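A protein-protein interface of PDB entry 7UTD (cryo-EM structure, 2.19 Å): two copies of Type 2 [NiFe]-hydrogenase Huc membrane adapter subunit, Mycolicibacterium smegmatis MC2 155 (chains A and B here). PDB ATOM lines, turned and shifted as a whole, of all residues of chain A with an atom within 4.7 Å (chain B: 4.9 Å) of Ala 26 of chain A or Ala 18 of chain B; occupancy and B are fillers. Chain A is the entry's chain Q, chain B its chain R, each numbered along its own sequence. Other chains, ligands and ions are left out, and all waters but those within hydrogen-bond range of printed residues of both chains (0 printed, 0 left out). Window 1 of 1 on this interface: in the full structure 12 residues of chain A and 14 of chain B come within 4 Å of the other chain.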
ATOM      1  N   LEU A  22      21.650   9.772  -4.819  1.00  0.00           N
ATOM      2  CA  LEU A  22      21.102   9.722  -3.445  1.00  0.00           C
ATOM      3  C   LEU A  22      22.179  10.263  -2.502  1.00  0.00           C
ATOM      4  O   LEU A  22      21.836  11.037  -1.609  1.00  0.00           O
ATOM      5  CB  LEU A  22      20.731   8.279  -3.101  1.00  0.00           C
ATOM      6  CG  LEU A  22      19.239   7.971  -2.982  1.00  0.00           C
ATOM      7  CD1 LEU A  22      18.390   9.210  -3.217  1.00  0.00           C
ATOM      8  CD2 LEU A  22      18.836   6.852  -3.929  1.00  0.00           C
ATOM      9  N   LEU A  23      23.428   9.898  -2.741  1.00  0.00           N
ATOM     10  CA  LEU A  23      24.503  10.317  -1.824  1.00  0.00           C
ATOM     11  C   LEU A  23      24.829  11.777  -2.105  1.00  0.00           C
ATOM     12  O   LEU A  23      25.448  12.408  -1.249  1.00  0.00           O
ATOM     13  CB  LEU A  23      25.711   9.407  -2.029  1.00  0.00           C
ATOM     14  CG  LEU A  23      25.487   7.939  -1.680  1.00  0.00           C
ATOM     15  CD1 LEU A  23      26.675   7.094  -2.097  1.00  0.00           C
ATOM     16  CD2 LEU A  23      25.202   7.774  -0.200  1.00  0.00           C
ATOM     17  N   ASP A  24      24.395  12.299  -3.245  1.00  0.00           N
ATOM     18  CA  ASP A  24      24.607  13.737  -3.541  1.00  0.00           C
ATOM     19  C   ASP A  24      23.659  14.551  -2.669  1.00  0.00           C
ATOM     20  O   ASP A  24      24.045  15.647  -2.251  1.00  0.00           O
ATOM     21  CB  ASP A  24      24.310  14.051  -5.003  1.00  0.00           C
ATOM     22  CG  ASP A  24      25.337  13.526  -5.985  1.00  0.00           C
ATOM     23  OD1 ASP A  24      26.403  13.088  -5.536  1.00  0.00           O
ATOM     24  OD2 ASP A  24      25.053  13.556  -7.196  1.00  0.00           O
ATOM     25  N   HIS A  25      22.476  14.018  -2.400  1.00  0.00           N
ATOM     26  CA  HIS A  25      21.445  14.740  -1.616  1.00  0.00           C
ATOM     27  C   HIS A  25      21.292  14.100  -0.235  1.00  0.00           C
ATOM     28  O   HIS A  25      20.267  14.337   0.411  1.00  0.00           O
ATOM     29  CB  HIS A  25      20.137  14.773  -2.410  1.00  0.00           C
ATOM     30  CG  HIS A  25      20.299  15.343  -3.776  1.00  0.00           C
ATOM     31  ND1 HIS A  25      20.027  14.616  -4.914  1.00  0.00           N
ATOM     32  CD2 HIS A  25      20.713  16.559  -4.190  1.00  0.00           C
ATOM     33  CE1 HIS A  25      20.266  15.357  -5.973  1.00  0.00           C
ATOM     34  NE2 HIS A  25      20.684  16.557  -5.556  1.00  0.00           N
ATOM     35  N   ALA A  26      22.265  13.289   0.170  1.00  0.00           N
ATOM     36  CA  ALA A  26      22.219  12.647   1.500  1.00  0.00           C
ATOM     37  C   ALA A  26      22.159  13.726   2.583  1.00  0.00           C
ATOM     38  O   ALA A  26      21.514  13.475   3.583  1.00  0.00           O
ATOM     39  CB  ALA A  26      23.399  11.736   1.684  1.00  0.00           C
ATOM     40  N   ASP A  27      22.816  14.866   2.376  1.00  0.00           N
ATOM     41  CA  ASP A  27      22.717  16.002   3.334  1.00  0.00           C
ATOM     42  C   ASP A  27      21.247  16.395   3.551  1.00  0.00           C
ATOM     43  O   ASP A  27      20.857  16.550   4.700  1.00  0.00           O
ATOM     44  CB  ASP A  27      23.589  17.180   2.896  1.00  0.00           C
ATOM     45  CG  ASP A  27      23.644  17.393   1.391  1.00  0.00           C
ATOM     46  OD1 ASP A  27      22.571  17.450   0.760  1.00  0.00           O
ATOM     47  OD2 ASP A  27      24.767  17.513   0.861  1.00  0.00           O
ATOM     48  N   LEU A  28      20.471  16.542   2.475  1.00  0.00           N
ATOM     49  CA  LEU A  28      19.032  16.887   2.575  1.00  0.00           C
ATOM     50  C   LEU A  28      18.289  15.775   3.317  1.00  0.00           C
ATOM     51  O   LEU A  28      17.512  16.092   4.206  1.00  0.00           O
ATOM     52  CB  LEU A  28      18.459  17.095   1.169  1.00  0.00           C
ATOM     53  CG  LEU A  28      16.956  17.347   1.099  1.00  0.00           C
ATOM     54  CD1 LEU A  28      16.607  18.689   1.723  1.00  0.00           C
ATOM     55  CD2 LEU A  28      16.463  17.277  -0.337  1.00  0.00           C
ATOM     56  N   LEU A  29      18.554  14.516   2.964  1.00  0.00           N
ATOM     57  CA  LEU A  29      17.926  13.397   3.708  1.00  0.00           C
ATOM     58  C   LEU A  29      18.321  13.504   5.183  1.00  0.00           C
ATOM     59  O   LEU A  29      17.423  13.469   6.017  1.00  0.00           O
ATOM     60  CB  LEU A  29      18.326  12.063   3.074  1.00  0.00           C
ATOM     61  CG  LEU A  29      17.992  11.937   1.588  1.00  0.00           C
ATOM     62  CD1 LEU A  29      18.612  10.684   0.990  1.00  0.00           C
ATOM     63  CD2 LEU A  29      16.489  11.952   1.366  1.00  0.00           C
ATOM     64  N   ALA A  30      19.611  13.671   5.470  1.00  0.00           N
ATOM     65  CA  ALA A  30      20.097  13.785   6.857  1.00  0.00           C
ATOM     66  C   ALA A  30      19.339  14.911   7.559  1.00  0.00           C
ATOM     67  O   ALA A  30      18.799  14.652   8.635  1.00  0.00           O
ATOM     68  CB  ALA A  30      21.580  14.031   6.860  1.00  0.00           C
ATOM     69  N   GLN B  14      31.473  15.555   3.402  1.00  0.00           N
ATOM     70  CA  GLN B  14      30.054  15.990   3.493  1.00  0.00           C
ATOM     71  C   GLN B  14      29.122  14.783   3.359  1.00  0.00           C
ATOM     72  O   GLN B  14      28.172  14.686   4.157  1.00  0.00           O
ATOM     73  CB  GLN B  14      29.783  17.036   2.413  1.00  0.00           C
ATOM     74  CG  GLN B  14      28.337  17.504   2.352  1.00  0.00           C
ATOM     75  CD  GLN B  14      27.759  17.367   0.965  1.00  0.00           C
ATOM     76  OE1 GLN B  14      26.897  18.139   0.551  1.00  0.00           O
ATOM     77  NE2 GLN B  14      28.236  16.375   0.230  1.00  0.00           N
ATOM     78  N   VAL B  15      29.390  13.892   2.405  1.00  0.00           N
ATOM     79  CA  VAL B  15      28.565  12.657   2.269  1.00  0.00           C
ATOM     80  C   VAL B  15      28.682  11.869   3.566  1.00  0.00           C
ATOM     81  O   VAL B  15      27.653  11.449   4.096  1.00  0.00           O
ATOM     82  CB  VAL B  15      28.990  11.799   1.068  1.00  0.00           C
ATOM     83  CG1 VAL B  15      28.332  10.432   1.079  1.00  0.00           C
ATOM     84  CG2 VAL B  15      28.709  12.508  -0.242  1.00  0.00           C
ATOM     85  N   ALA B  16      29.899  11.697   4.056  1.00  0.00           N
ATOM     86  CA  ALA B  16      30.101  10.901   5.280  1.00  0.00           C
ATOM     87  C   ALA B  16      29.327  11.538   6.425  1.00  0.00           C
ATOM     88  O   ALA B  16      28.663  10.804   7.163  1.00  0.00           O
ATOM     89  CB  ALA B  16      31.561  10.859   5.596  1.00  0.00           C
ATOM     90  N   GLU B  17      29.443  12.853   6.574  1.00  0.00           N
ATOM     91  CA  GLU B  17      28.746  13.568   7.671  1.00  0.00           C
ATOM     92  C   GLU B  17      27.249  13.256   7.611  1.00  0.00           C
ATOM     93  O   GLU B  17      26.696  12.878   8.650  1.00  0.00           O
ATOM     94  CB  GLU B  17      29.036  15.062   7.557  1.00  0.00           C
ATOM     95  CG  GLU B  17      28.157  15.934   8.430  1.00  0.00           C
ATOM     96  CD  GLU B  17      28.318  17.416   8.146  1.00  0.00           C
ATOM     97  OE1 GLU B  17      29.052  17.754   7.195  1.00  0.00           O
ATOM     98  OE2 GLU B  17      27.713  18.226   8.874  1.00  0.00           O
ATOM     99  N   ALA B  18      26.638  13.382   6.432  1.00  0.00           N
ATOM    100  CA  ALA B  18      25.190  13.131   6.267  1.00  0.00           C
ATOM    101  C   ALA B  18      24.856  11.670   6.581  1.00  0.00           C
ATOM    102  O   ALA B  18      23.864  11.439   7.277  1.00  0.00           O
ATOM    103  CB  ALA B  18      24.747  13.516   4.878  1.00  0.00           C
ATOM    104  N   LEU B  19      25.660  10.733   6.080  1.00  0.00           N
ATOM    105  CA  LEU B  19      25.412   9.288   6.319  1.00  0.00           C
ATOM    106  C   LEU B  19      25.539   8.999   7.812  1.00  0.00           C
ATOM    107  O   LEU B  19      24.747   8.206   8.309  1.00  0.00           O
ATOM    108  CB  LEU B  19      26.393   8.446   5.502  1.00  0.00           C
ATOM    109  CG  LEU B  19      25.806   7.749   4.277  1.00  0.00           C
ATOM    110  CD1 LEU B  19      24.442   8.317   3.920  1.00  0.00           C
ATOM    111  CD2 LEU B  19      26.749   7.858   3.093  1.00  0.00           C
ATOM    112  N   ASN B  20      26.471   9.663   8.482  1.00  0.00           N
ATOM    113  CA  ASN B  20      26.647   9.478   9.941  1.00  0.00           C
ATOM    114  C   ASN B  20      25.416  10.021  10.665  1.00  0.00           C
ATOM    115  O   ASN B  20      24.965   9.364  11.606  1.00  0.00           O
ATOM    116  CB  ASN B  20      27.927  10.138  10.445  1.00  0.00           C
ATOM    117  CG  ASN B  20      29.179   9.435   9.970  1.00  0.00           C
ATOM    118  OD1 ASN B  20      29.182   8.221   9.794  1.00  0.00           O
ATOM    119  ND2 ASN B  20      30.245  10.189   9.764  1.00  0.00           N
ATOM    120  N   SER B  21      24.899  11.170  10.234  1.00  0.00           N
ATOM    121  CA  SER B  21      23.701  11.767  10.870  1.00  0.00           C
ATOM    122  C   SER B  21      22.491  10.877  10.604  1.00  0.00           C
ATOM    123  O   SER B  21      21.596  10.836  11.461  1.00  0.00           O
ATOM    124  CB  SER B  21      23.471  13.189  10.422  1.00  0.00           C
ATOM    125  OG  SER B  21      22.247  13.308   9.715  1.00  0.00           O
ATOM    126  N   LEU B  22      22.479  10.226   9.450  1.00  0.00           N
ATOM    127  CA  LEU B  22      21.350   9.342   9.114  1.00  0.00           C
ATOM    128  C   LEU B  22      21.429   8.173  10.083  1.00  0.00           C
ATOM    129  O   LEU B  22      20.394   7.773  10.606  1.00  0.00           O
ATOM    130  CB  LEU B  22      21.512   8.892   7.665  1.00  0.00           C
ATOM    131  CG  LEU B  22      20.387   9.277   6.708  1.00  0.00           C
ATOM    132  CD1 LEU B  22      19.438  10.268   7.353  1.00  0.00           C
ATOM    133  CD2 LEU B  22      20.946   9.833   5.409  1.00  0.00           C
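Position printed for both chains: 22.
Of the 8 pairs that touch across the chains among the printed residues, none has its exchanged pair printed and touching as well.
Hydrophobic or aromatic side chains of chain A that line the printed part of chain B: Leu 23, Ala 26 and Ala 30.
Among the printed residues, 8 pairs touch across the chains.
Among the printed residues, no Asp or Glu carboxylate lies within 4 Å of a Lys or Arg side-chain nitrogen of the other chain.
Leu 22 of chain A touches none of the printed residues of chain B.
Printed residues of chain B within 4 Å of Leu 23 of chain A: Val 15 and Leu 19.
Ala 26 of chain A touches one residue of chain B.
Leu 29 of chain A touches none of the printed residues of chain B.
Of the printed residues of chain A, Val 15 of chain B touches Leu 23.
Ala 18 of chain B touches just these residues of chain A: Ala 26 (3.5 Å), Asp 27 (3.4 Å) and Ala 30 (3.5 Å).
Of the printed residues of chain A, Ser 21 of chain B touches Ala 30.
Printed residues of chain A within 4 Å of Leu 22 of chain B: Ala 30 (3.6 Å).
The nearest printed residue of chain A that does not touch Val 15 of chain B is Ala 26 of chain A (4.9 Å).
The side-chain hydroxyl (OG) of Ser 21 of chain B lies within hydrogen-bond range of the backbone carbonyl oxygen (O) of Ala 18 of chain B, 3.5 Å away.
OE1 of Gln 14 of chain B lies close to OD2 of Asp 27 of chain A, 2.2 Å away.
Leu 23 of chain A touches Val 15 of chain B (O to CG2, 3.4 Å).
CD2 of Leu 23 of chain A touches CD2 of Leu 19 of chain B (3.6 Å).
Ala 18 of chain B touches Ala 26 of chain A (CB to C, 3.5 Å).
Ala 18 of chain B touches Asp 27 of chain A (CB to N, 3.4 Å).
CB of Ala 30 of chain A touches O of Ala 18 of chain B, 3.5 Å away.
Ala 30 of chain A touches Ser 21 of chain B (CB to OG, 3.0 Å).
CD1 of Leu 22 of chain B touches CA of Ala 30 of chain A, at 3.6 Å.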
